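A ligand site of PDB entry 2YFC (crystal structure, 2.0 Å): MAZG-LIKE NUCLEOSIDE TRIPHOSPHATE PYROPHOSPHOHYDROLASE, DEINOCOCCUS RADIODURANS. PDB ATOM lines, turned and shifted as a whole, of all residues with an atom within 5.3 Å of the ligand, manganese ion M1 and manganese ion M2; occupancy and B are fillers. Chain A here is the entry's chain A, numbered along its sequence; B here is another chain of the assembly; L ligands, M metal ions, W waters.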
ATOM      1  N   VAL A 111       6.742 -22.557   3.001  1.00  0.00           N
ATOM      2  CA  VAL A 111       5.748 -22.812   1.955  1.00  0.00           C
ATOM      3  C   VAL A 111       4.338 -23.056   2.548  1.00  0.00           C
ATOM      4  O   VAL A 111       3.344 -22.536   2.029  1.00  0.00           O
ATOM      5  CB  VAL A 111       6.211 -24.000   1.064  1.00  0.00           C
ATOM      6  CG1 VAL A 111       5.063 -24.521   0.189  1.00  0.00           C
ATOM      7  CG2 VAL A 111       7.404 -23.569   0.220  1.00  0.00           C
ATOM      8  N   ASN A 115       0.752 -20.990   2.063  1.00  0.00           N
ATOM      9  CA  ASN A 115      -0.385 -21.731   1.560  1.00  0.00           C
ATOM     10  C   ASN A 115      -1.640 -21.504   2.404  1.00  0.00           C
ATOM     11  O   ASN A 115      -2.689 -21.420   1.900  1.00  0.00           O
ATOM     12  CB  ASN A 115      -0.056 -23.188   1.380  1.00  0.00           C
ATOM     13  CG  ASN A 115       0.707 -23.442   0.072  1.00  0.00           C
ATOM     14  OD1 ASN A 115       0.756 -22.624  -0.730  1.00  0.00           O
ATOM     15  ND2 ASN A 115       1.256 -24.581  -0.069  1.00  0.00           N
ATOM     16  N   LYS A 118      -3.717 -18.505   1.610  1.00  0.00           N
ATOM     17  CA  LYS A 118      -4.523 -18.504   0.390  1.00  0.00           C
ATOM     18  C   LYS A 118      -6.012 -18.733   0.660  1.00  0.00           C
ATOM     19  O   LYS A 118      -6.834 -18.641  -0.252  1.00  0.00           O
ATOM     20  CB  LYS A 118      -4.041 -19.572  -0.594  1.00  0.00           C
ATOM     21  CG  LYS A 118      -2.642 -19.358  -1.147  1.00  0.00           C
ATOM     22  CD  LYS A 118      -2.165 -20.603  -1.946  1.00  0.00           C
ATOM     23  CE  LYS A 118      -0.739 -20.380  -2.507  1.00  0.00           C
ATOM     24  NZ  LYS A 118      -0.225 -21.568  -3.302  1.00  0.00           N
ATOM     25  N   GLY A 127     -10.975 -27.362  -8.919  1.00  0.00           N
ATOM     26  CA  GLY A 127     -10.863 -27.419  -7.468  1.00  0.00           C
ATOM     27  C   GLY A 127      -9.570 -26.851  -6.902  1.00  0.00           C
ATOM     28  O   GLY A 127      -9.390 -26.796  -5.686  1.00  0.00           O
ATOM     29  N   LYS A 128      -8.672 -26.421  -7.776  1.00  0.00           N
ATOM     30  CA  LYS A 128      -7.417 -25.849  -7.294  1.00  0.00           C
ATOM     31  C   LYS A 128      -7.671 -24.542  -6.562  1.00  0.00           C
ATOM     32  O   LYS A 128      -8.400 -23.668  -7.033  1.00  0.00           O
ATOM     33  CB  LYS A 128      -6.399 -25.601  -8.419  1.00  0.00           C
ATOM     34  CG  LYS A 128      -5.064 -25.008  -7.902  1.00  0.00           C
ATOM     35  CD  LYS A 128      -4.088 -24.676  -9.036  1.00  0.00           C
ATOM     36  CE  LYS A 128      -2.726 -24.233  -8.491  1.00  0.00           C
ATOM     37  NZ  LYS A 128      -1.757 -23.944  -9.586  1.00  0.00           N
ATOM     38  N   GLN A 129      -7.055 -24.419  -5.388  1.00  0.00           N
ATOM     39  CA  GLN A 129      -7.133 -23.180  -4.621  1.00  0.00           C
ATOM     40  C   GLN A 129      -6.220 -22.122  -5.237  1.00  0.00           C
ATOM     41  O   GLN A 129      -5.037 -22.387  -5.484  1.00  0.00           O
ATOM     42  CB  GLN A 129      -6.693 -23.446  -3.166  1.00  0.00           C
ATOM     43  CG  GLN A 129      -6.652 -22.192  -2.316  1.00  0.00           C
ATOM     44  CD  GLN A 129      -8.014 -21.581  -2.155  1.00  0.00           C
ATOM     45  OE1 GLN A 129      -8.973 -22.421  -1.774  1.00  0.00           O
ATOM     46  NE2 GLN A 129      -8.224 -20.400  -2.411  1.00  0.00           N
ATOM     47  N   LYS A 131      -4.868 -17.799  -5.462  1.00  0.00           N
ATOM     48  CA  LYS A 131      -4.328 -16.789  -4.549  1.00  0.00           C
ATOM     49  C   LYS A 131      -5.264 -15.573  -4.469  1.00  0.00           C
ATOM     50  O   LYS A 131      -5.707 -15.082  -5.493  1.00  0.00           O
ATOM     51  CB  LYS A 131      -2.944 -16.368  -5.059  1.00  0.00           C
ATOM     52  CG  LYS A 131      -1.936 -17.522  -5.006  1.00  0.00           C
ATOM     53  CD  LYS A 131      -0.788 -17.364  -6.023  1.00  0.00           C
ATOM     54  CE  LYS A 131       0.107 -18.619  -5.988  1.00  0.00           C
ATOM     55  NZ  LYS A 131       1.052 -18.697  -7.144  1.00  0.00           N
ATOM     56  N   LEU B  20      -0.702 -30.639   5.861  1.00  0.00           N
ATOM     57  CA  LEU B  20      -1.628 -30.722   4.728  1.00  0.00           C
ATOM     58  C   LEU B  20      -3.064 -30.809   5.234  1.00  0.00           C
ATOM     59  O   LEU B  20      -3.979 -30.201   4.677  1.00  0.00           O
ATOM     60  CB  LEU B  20      -1.317 -31.910   3.810  1.00  0.00           C
ATOM     61  CG  LEU B  20      -0.648 -31.536   2.473  1.00  0.00           C
ATOM     62  CD1 LEU B  20      -1.531 -30.552   1.687  1.00  0.00           C
ATOM     63  CD2 LEU B  20       0.708 -30.926   2.747  1.00  0.00           C
ATOM     64  N   PHE B  23      -4.103 -27.439   6.093  1.00  0.00           N
ATOM     65  CA  PHE B  23      -4.401 -26.688   4.865  1.00  0.00           C
ATOM     66  C   PHE B  23      -5.764 -27.028   4.254  1.00  0.00           C
ATOM     67  O   PHE B  23      -6.555 -26.129   3.935  1.00  0.00           O
ATOM     68  CB  PHE B  23      -3.274 -26.922   3.838  1.00  0.00           C
ATOM     69  CG  PHE B  23      -3.549 -26.322   2.476  1.00  0.00           C
ATOM     70  CD1 PHE B  23      -3.533 -24.936   2.293  1.00  0.00           C
ATOM     71  CD2 PHE B  23      -3.793 -27.132   1.386  1.00  0.00           C
ATOM     72  CE1 PHE B  23      -3.771 -24.380   1.038  1.00  0.00           C
ATOM     73  CE2 PHE B  23      -4.026 -26.590   0.130  1.00  0.00           C
ATOM     74  CZ  PHE B  23      -4.020 -25.206  -0.050  1.00  0.00           C
ATOM     75  N   HIS B  24      -6.049 -28.309   4.098  1.00  0.00           N
ATOM     76  CA  HIS B  24      -7.324 -28.711   3.490  1.00  0.00           C
ATOM     77  C   HIS B  24      -8.549 -28.324   4.325  1.00  0.00           C
ATOM     78  O   HIS B  24      -9.585 -27.934   3.775  1.00  0.00           O
ATOM     79  CB  HIS B  24      -7.303 -30.195   3.130  1.00  0.00           C
ATOM     80  CG  HIS B  24      -6.441 -30.482   1.931  1.00  0.00           C
ATOM     81  ND1 HIS B  24      -5.890 -31.720   1.679  1.00  0.00           N
ATOM     82  CD2 HIS B  24      -6.019 -29.668   0.937  1.00  0.00           C
ATOM     83  CE1 HIS B  24      -5.180 -31.660   0.557  1.00  0.00           C
ATOM     84  NE2 HIS B  24      -5.240 -30.426   0.094  1.00  0.00           N
ATOM     85  N   ILE B  27      -9.156 -24.586   3.676  1.00  0.00           N
ATOM     86  CA  ILE B  27      -9.696 -24.203   2.385  1.00  0.00           C
ATOM     87  C   ILE B  27     -10.977 -24.954   2.051  1.00  0.00           C
ATOM     88  O   ILE B  27     -11.533 -24.791   0.971  1.00  0.00           O
ATOM     89  CB  ILE B  27      -8.663 -24.366   1.240  1.00  0.00           C
ATOM     90  CG1 ILE B  27      -8.378 -25.853   0.992  1.00  0.00           C
ATOM     91  CG2 ILE B  27      -7.365 -23.632   1.576  1.00  0.00           C
ATOM     92  CD1 ILE B  27      -7.641 -26.093  -0.316  1.00  0.00           C
ATOM     93  N   LEU B  45      -7.870 -33.829 -10.347  1.00  0.00           N
ATOM     94  CA  LEU B  45      -7.184 -32.689  -9.751  1.00  0.00           C
ATOM     95  C   LEU B  45      -5.811 -33.089  -9.228  1.00  0.00           C
ATOM     96  O   LEU B  45      -4.841 -32.373  -9.457  1.00  0.00           O
ATOM     97  CB  LEU B  45      -8.000 -32.030  -8.631  1.00  0.00           C
ATOM     98  CG  LEU B  45      -7.253 -30.934  -7.847  1.00  0.00           C
ATOM     99  CD1 LEU B  45      -7.028 -29.710  -8.728  1.00  0.00           C
ATOM    100  CD2 LEU B  45      -7.991 -30.550  -6.560  1.00  0.00           C
ATOM    101  N   ARG B  46      -5.703 -34.221  -8.520  1.00  0.00           N
ATOM    102  CA  ARG B  46      -4.393 -34.563  -7.956  1.00  0.00           C
ATOM    103  C   ARG B  46      -3.357 -34.743  -9.073  1.00  0.00           C
ATOM    104  O   ARG B  46      -2.203 -34.340  -8.938  1.00  0.00           O
ATOM    105  CB  ARG B  46      -4.423 -35.811  -7.037  1.00  0.00           C
ATOM    106  CG  ARG B  46      -5.384 -35.743  -5.832  1.00  0.00           C
ATOM    107  CD  ARG B  46      -5.446 -34.344  -5.194  1.00  0.00           C
ATOM    108  NE  ARG B  46      -4.139 -33.797  -4.824  1.00  0.00           N
ATOM    109  CZ  ARG B  46      -3.984 -32.732  -4.031  1.00  0.00           C
ATOM    110  NH1 ARG B  46      -5.057 -32.132  -3.506  1.00  0.00           N
ATOM    111  NH2 ARG B  46      -2.765 -32.263  -3.753  1.00  0.00           N
ATOM    112  N   LEU B  49      -2.199 -31.305 -10.454  1.00  0.00           N
ATOM    113  CA  LEU B  49      -1.284 -30.575  -9.567  1.00  0.00           C
ATOM    114  C   LEU B  49       0.093 -31.260  -9.541  1.00  0.00           C
ATOM    115  O   LEU B  49       1.113 -30.584  -9.505  1.00  0.00           O
ATOM    116  CB  LEU B  49      -1.874 -30.478  -8.156  1.00  0.00           C
ATOM    117  CG  LEU B  49      -3.219 -29.753  -8.028  1.00  0.00           C
ATOM    118  CD1 LEU B  49      -3.697 -29.781  -6.570  1.00  0.00           C
ATOM    119  CD2 LEU B  49      -3.133 -28.295  -8.557  1.00  0.00           C
ATOM    120  N   GLU B  52       1.731 -30.275 -12.813  1.00  0.00           N
ATOM    121  CA  GLU B  52       2.107 -28.866 -12.758  1.00  0.00           C
ATOM    122  C   GLU B  52       3.386 -28.617 -11.945  1.00  0.00           C
ATOM    123  O   GLU B  52       4.327 -27.967 -12.424  1.00  0.00           O
ATOM    124  CB  GLU B  52       0.963 -28.008 -12.210  1.00  0.00           C
ATOM    125  CG  GLU B  52       1.367 -26.546 -12.148  1.00  0.00           C
ATOM    126  CD  GLU B  52       0.395 -25.658 -11.357  1.00  0.00           C
ATOM    127  OE1 GLU B  52      -0.767 -26.054 -11.068  1.00  0.00           O
ATOM    128  OE2 GLU B  52       0.829 -24.539 -11.039  1.00  0.00           O
ATOM    129  N   GLU B  53       3.403 -29.086 -10.704  1.00  0.00           N
ATOM    130  CA  GLU B  53       4.537 -28.807  -9.826  1.00  0.00           C
ATOM    131  C   GLU B  53       5.805 -29.557 -10.240  1.00  0.00           C
ATOM    132  O   GLU B  53       6.915 -29.053 -10.062  1.00  0.00           O
ATOM    133  CB  GLU B  53       4.211 -29.065  -8.348  1.00  0.00           C
ATOM    134  CG  GLU B  53       3.058 -28.201  -7.820  1.00  0.00           C
ATOM    135  CD  GLU B  53       3.253 -26.725  -8.108  1.00  0.00           C
ATOM    136  OE1 GLU B  53       4.329 -26.156  -7.787  1.00  0.00           O
ATOM    137  OE2 GLU B  53       2.343 -26.127  -8.696  1.00  0.00           O
ATOM    138  N   GLU B  56       7.410 -27.617 -12.959  1.00  0.00           N
ATOM    139  CA  GLU B  56       8.141 -26.491 -12.376  1.00  0.00           C
ATOM    140  C   GLU B  56       9.498 -26.888 -11.789  1.00  0.00           C
ATOM    141  O   GLU B  56      10.470 -26.124 -11.886  1.00  0.00           O
ATOM    142  CB  GLU B  56       7.292 -25.779 -11.305  1.00  0.00           C
ATOM    143  CG  GLU B  56       6.070 -25.121 -11.909  1.00  0.00           C
ATOM    144  CD  GLU B  56       5.125 -24.547 -10.877  1.00  0.00           C
ATOM    145  OE1 GLU B  56       5.583 -24.051  -9.838  1.00  0.00           O
ATOM    146  OE2 GLU B  56       3.914 -24.576 -11.133  1.00  0.00           O
ATOM    147  N   GLU B  85      10.306 -25.081  -5.460  1.00  0.00           N
ATOM    148  CA  GLU B  85       9.503 -25.966  -6.300  1.00  0.00           C
ATOM    149  C   GLU B  85       9.517 -27.412  -5.794  1.00  0.00           C
ATOM    150  O   GLU B  85       8.527 -28.119  -5.950  1.00  0.00           O
ATOM    151  CB  GLU B  85       9.933 -25.877  -7.773  1.00  0.00           C
ATOM    152  CG  GLU B  85       9.894 -24.447  -8.346  1.00  0.00           C
ATOM    153  CD  GLU B  85       8.513 -23.805  -8.252  1.00  0.00           C
ATOM    154  OE1 GLU B  85       7.581 -24.452  -7.775  1.00  0.00           O
ATOM    155  OE2 GLU B  85       8.370 -22.646  -8.676  1.00  0.00           O
ATOM    156  N   ALA B  87       9.639 -28.247  -2.637  1.00  0.00           N
ATOM    157  CA  ALA B  87       8.721 -28.179  -1.512  1.00  0.00           C
ATOM    158  C   ALA B  87       7.250 -28.143  -1.977  1.00  0.00           C
ATOM    159  O   ALA B  87       6.400 -28.779  -1.362  1.00  0.00           O
ATOM    160  CB  ALA B  87       9.034 -26.967  -0.648  1.00  0.00           C
ATOM    161  N   ASP B  88       6.983 -27.420  -3.060  1.00  0.00           N
ATOM    162  CA  ASP B  88       5.650 -27.457  -3.701  1.00  0.00           C
ATOM    163  C   ASP B  88       5.264 -28.863  -4.189  1.00  0.00           C
ATOM    164  O   ASP B  88       4.091 -29.263  -4.126  1.00  0.00           O
ATOM    165  CB  ASP B  88       5.603 -26.487  -4.908  1.00  0.00           C
ATOM    166  CG  ASP B  88       5.284 -25.057  -4.503  1.00  0.00           C
ATOM    167  OD1 ASP B  88       5.079 -24.781  -3.288  1.00  0.00           O
ATOM    168  OD2 ASP B  88       5.212 -24.193  -5.400  1.00  0.00           O
ATOM    169  N   TYR B  91       4.374 -30.844  -1.331  1.00  0.00           N
ATOM    170  CA  TYR B  91       3.093 -30.371  -0.803  1.00  0.00           C
ATOM    171  C   TYR B  91       1.894 -31.004  -1.538  1.00  0.00           C
ATOM    172  O   TYR B  91       0.918 -31.420  -0.907  1.00  0.00           O
ATOM    173  CB  TYR B  91       3.063 -28.850  -0.839  1.00  0.00           C
ATOM    174  CG  TYR B  91       2.176 -28.200   0.221  1.00  0.00           C
ATOM    175  CD1 TYR B  91       0.793 -28.065   0.017  1.00  0.00           C
ATOM    176  CD2 TYR B  91       2.712 -27.679   1.399  1.00  0.00           C
ATOM    177  CE1 TYR B  91      -0.015 -27.470   0.979  1.00  0.00           C
ATOM    178  CE2 TYR B  91       1.903 -27.077   2.368  1.00  0.00           C
ATOM    179  CZ  TYR B  91       0.538 -26.980   2.144  1.00  0.00           C
ATOM    180  OH  TYR B  91      -0.265 -26.388   3.083  1.00  0.00           O
ATOM    181  N   VAL B  92       1.958 -31.091  -2.857  1.00  0.00           N
ATOM    182  CA  VAL B  92       0.858 -31.706  -3.607  1.00  0.00           C
ATOM    183  C   VAL B  92       0.887 -33.244  -3.557  1.00  0.00           C
ATOM    184  O   VAL B  92      -0.125 -33.887  -3.824  1.00  0.00           O
ATOM    185  CB  VAL B  92       0.777 -31.227  -5.087  1.00  0.00           C
ATOM    186  CG1 VAL B  92       0.567 -29.746  -5.143  1.00  0.00           C
ATOM    187  CG2 VAL B  92       2.036 -31.657  -5.896  1.00  0.00           C
HETATM  188  N1  LIG L   1      -1.654 -25.987  -3.409  1.00  0.00           N
HETATM  189  C1  LIG L   1      -2.302 -27.083  -2.983  1.00  0.00           C
HETATM  190  N2  LIG L   1      -3.642 -27.290  -3.363  1.00  0.00           N
HETATM  191  C2  LIG L   1      -4.280 -26.368  -4.172  1.00  0.00           C
HETATM  192  C3  LIG L   1      -3.616 -25.225  -4.639  1.00  0.00           C
HETATM  193  C4  LIG L   1      -2.307 -25.028  -4.264  1.00  0.00           C
HETATM  194  O1  LIG L   1      -1.740 -27.907  -2.277  1.00  0.00           O
HETATM  195  O2  LIG L   1      -5.586 -26.612  -4.518  1.00  0.00           O
HETATM  196  C5  LIG L   1      -0.264 -25.785  -3.051  1.00  0.00           C
HETATM  197  C6  LIG L   1       0.917 -26.683  -3.521  1.00  0.00           C
HETATM  198  C7  LIG L   1       2.059 -25.743  -3.654  1.00  0.00           C
HETATM  199  C8  LIG L   1       1.330 -24.532  -4.212  1.00  0.00           C
HETATM  200  O3  LIG L   1       2.820 -25.593  -2.516  1.00  0.00           O
HETATM  201  O4  LIG L   1       0.227 -24.385  -3.281  1.00  0.00           O
HETATM  202  C9  LIG L   1       0.986 -24.414  -5.666  1.00  0.00           C
HETATM  203  O5  LIG L   1       0.467 -23.130  -5.696  1.00  0.00           O
HETATM  204  P1  LIG L   1       0.572 -22.407  -7.083  1.00  0.00           P
HETATM  205  O6  LIG L   1       0.686 -23.352  -8.236  1.00  0.00           O
HETATM  206  O7  LIG L   1       1.797 -21.549  -7.034  1.00  0.00           O
HETATM  207  O8  LIG L   1      -0.688 -21.632  -7.350  1.00  0.00           O
HETATM  208 MN    MN M   1       2.349 -24.028  -9.559  1.00  0.00          MN
HETATM  209 MN    MN M   2       5.343 -24.316  -7.640  1.00  0.00          MN
HETATM  210  O   HOH W   1      -2.425 -21.473  -5.254  1.00  0.00           O
HETATM  211  O   HOH W   2       3.724 -23.054  -8.174  1.00  0.00           O
HETATM  212  O   HOH W   3      -1.691 -19.954  -9.056  1.00  0.00           O
HETATM  213  O   HOH W   4       2.188 -20.976  -4.439  1.00  0.00           O
HETATM  214  O   HOH W   5      -2.432 -30.346  -1.748  1.00  0.00           O
HETATM  215  O   HOH W   6      -7.604 -28.272  -3.372  1.00  0.00           O
HETATM  216  O   HOH W   7       6.028 -21.490  -6.165  1.00  0.00           O
HETATM  217  O   HOH W   8       2.214 -21.856 -10.624  1.00  0.00           O
HETATM  218  O   HOH W   9      -5.284 -29.372  -2.547  1.00  0.00           O
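The side-chain amino group of Lys 131 lies within salt-bridge range of an oxygen (O7) of the ligand, 2.9 Å away. NZ of Lys 118 lies within hydrogen-bond range of O4 of the ligand (2.9 Å). The side-chain amide nitrogen of Asn 115 lies within hydrogen-bond range of an oxygen (O3) of the ligand. N of Gln 129 sits at hydrogen-bond distance from O2 of the ligand (2.8 Å). An oxygen (O3) of the ligand sits at hydrogen-bond distance from the side-chain carboxylate (OD1) of Asp 88 of chain B (2.5 Å). O8 of the ligand lies within salt-bridge range of NZ of Lys 128, 3.4 Å away.
The nearest printed residue that does not touch manganese ion M2 is Glu 52 of chain B (5.7 Å).
Residues that only touch the ligand: Tyr 91 of chain B (3.4 Å), Val 92 of chain B (3.5 Å), Phe 23 of chain B (3.6 Å), Val 111 (3.7 Å) and Gly 127 (3.98 Å). Within 4 Å of the ligand: Val 111, Asn 115, Lys 118, Gly 127, Lys 128, Gln 129, Lys 131, Phe 23 of chain B, Glu 52 of chain B, Glu 53 of chain B, Asp 88 of chain B, Tyr 91 of chain B and Val 92 of chain B. The nearest printed residue that does not touch the ligand is Leu 49 of chain B (4.1 Å).
Water W2 binds manganese ion M1 (2.2 Å). OE2 of Glu 52 of chain B is bound to manganese ion M1 (2.2 Å). Manganese ion M1 is bound by O6 of the ligand, 2.2 Å away. OE2 of Glu 53 of chain B binds manganese ion M1, at 2.3 Å. The side-chain carboxylate (OE2) of Glu 56 of chain B is bound to manganese ion M1 (2.3 Å). Water W8 binds manganese ion M1 (2.4 Å). Manganese ion M1 has six donor atoms within binding distance.
The side-chain amide nitrogen of Gln 129 is in hydrogen-bond range of the backbone carbonyl oxygen of Lys 118 (3.1 Å). NZ of Lys 118 is in hydrogen-bond range of OD1 of Asn 115 (2.9 Å). The side-chain amino group of Lys 128 lies within salt-bridge range of the side-chain carboxylate of Glu 52 of chain B (2.8 Å). The guanidinium group of Arg 46 of chain B sits at hydrogen-bond distance from the backbone carbonyl oxygen of Val 92 of chain B (3.1 Å).
Water W5 lies within hydrogen-bond range of O1 of the ligand (2.6 Å), NH2 of Arg 46 of chain B (2.8 Å) and NE2 of His 24 of chain B (3.4 Å). Water W4 lies within hydrogen-bond range of an oxygen (O7) of the ligand (2.7 Å) and the side-chain amino group (NZ) of Lys 118 (2.7 Å). Water W1 lies within hydrogen-bond range of an oxygen (O8) of the ligand, the backbone carbonyl oxygen of Gln 129 and the side-chain amino group of Lys 118. Water W9 lies within hydrogen-bond range of a nitrogen (N2) of the ligand (2.8 Å), a ring nitrogen (NE2) of His 24 of chain B (2.8 Å) and the guanidinium group (NH1) of Arg 46 of chain B (2.9 Å). Water W6 bridges O2 of the ligand (2.9 Å) and O of Gly 127 (3.3 Å).
Manganese ion M2 is bound by the side-chain carboxylate of Glu 53 of chain B (2.1 Å), water W2 (2.1 Å), the side-chain carboxylate of Glu 56 of chain B (2.2 Å), the side-chain carboxylate of Glu 85 of chain B (2.2 Å) and the side-chain carboxylate of Asp 88 of chain B (2.2 Å). Manganese ion M2 has five donor atoms within binding distance.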
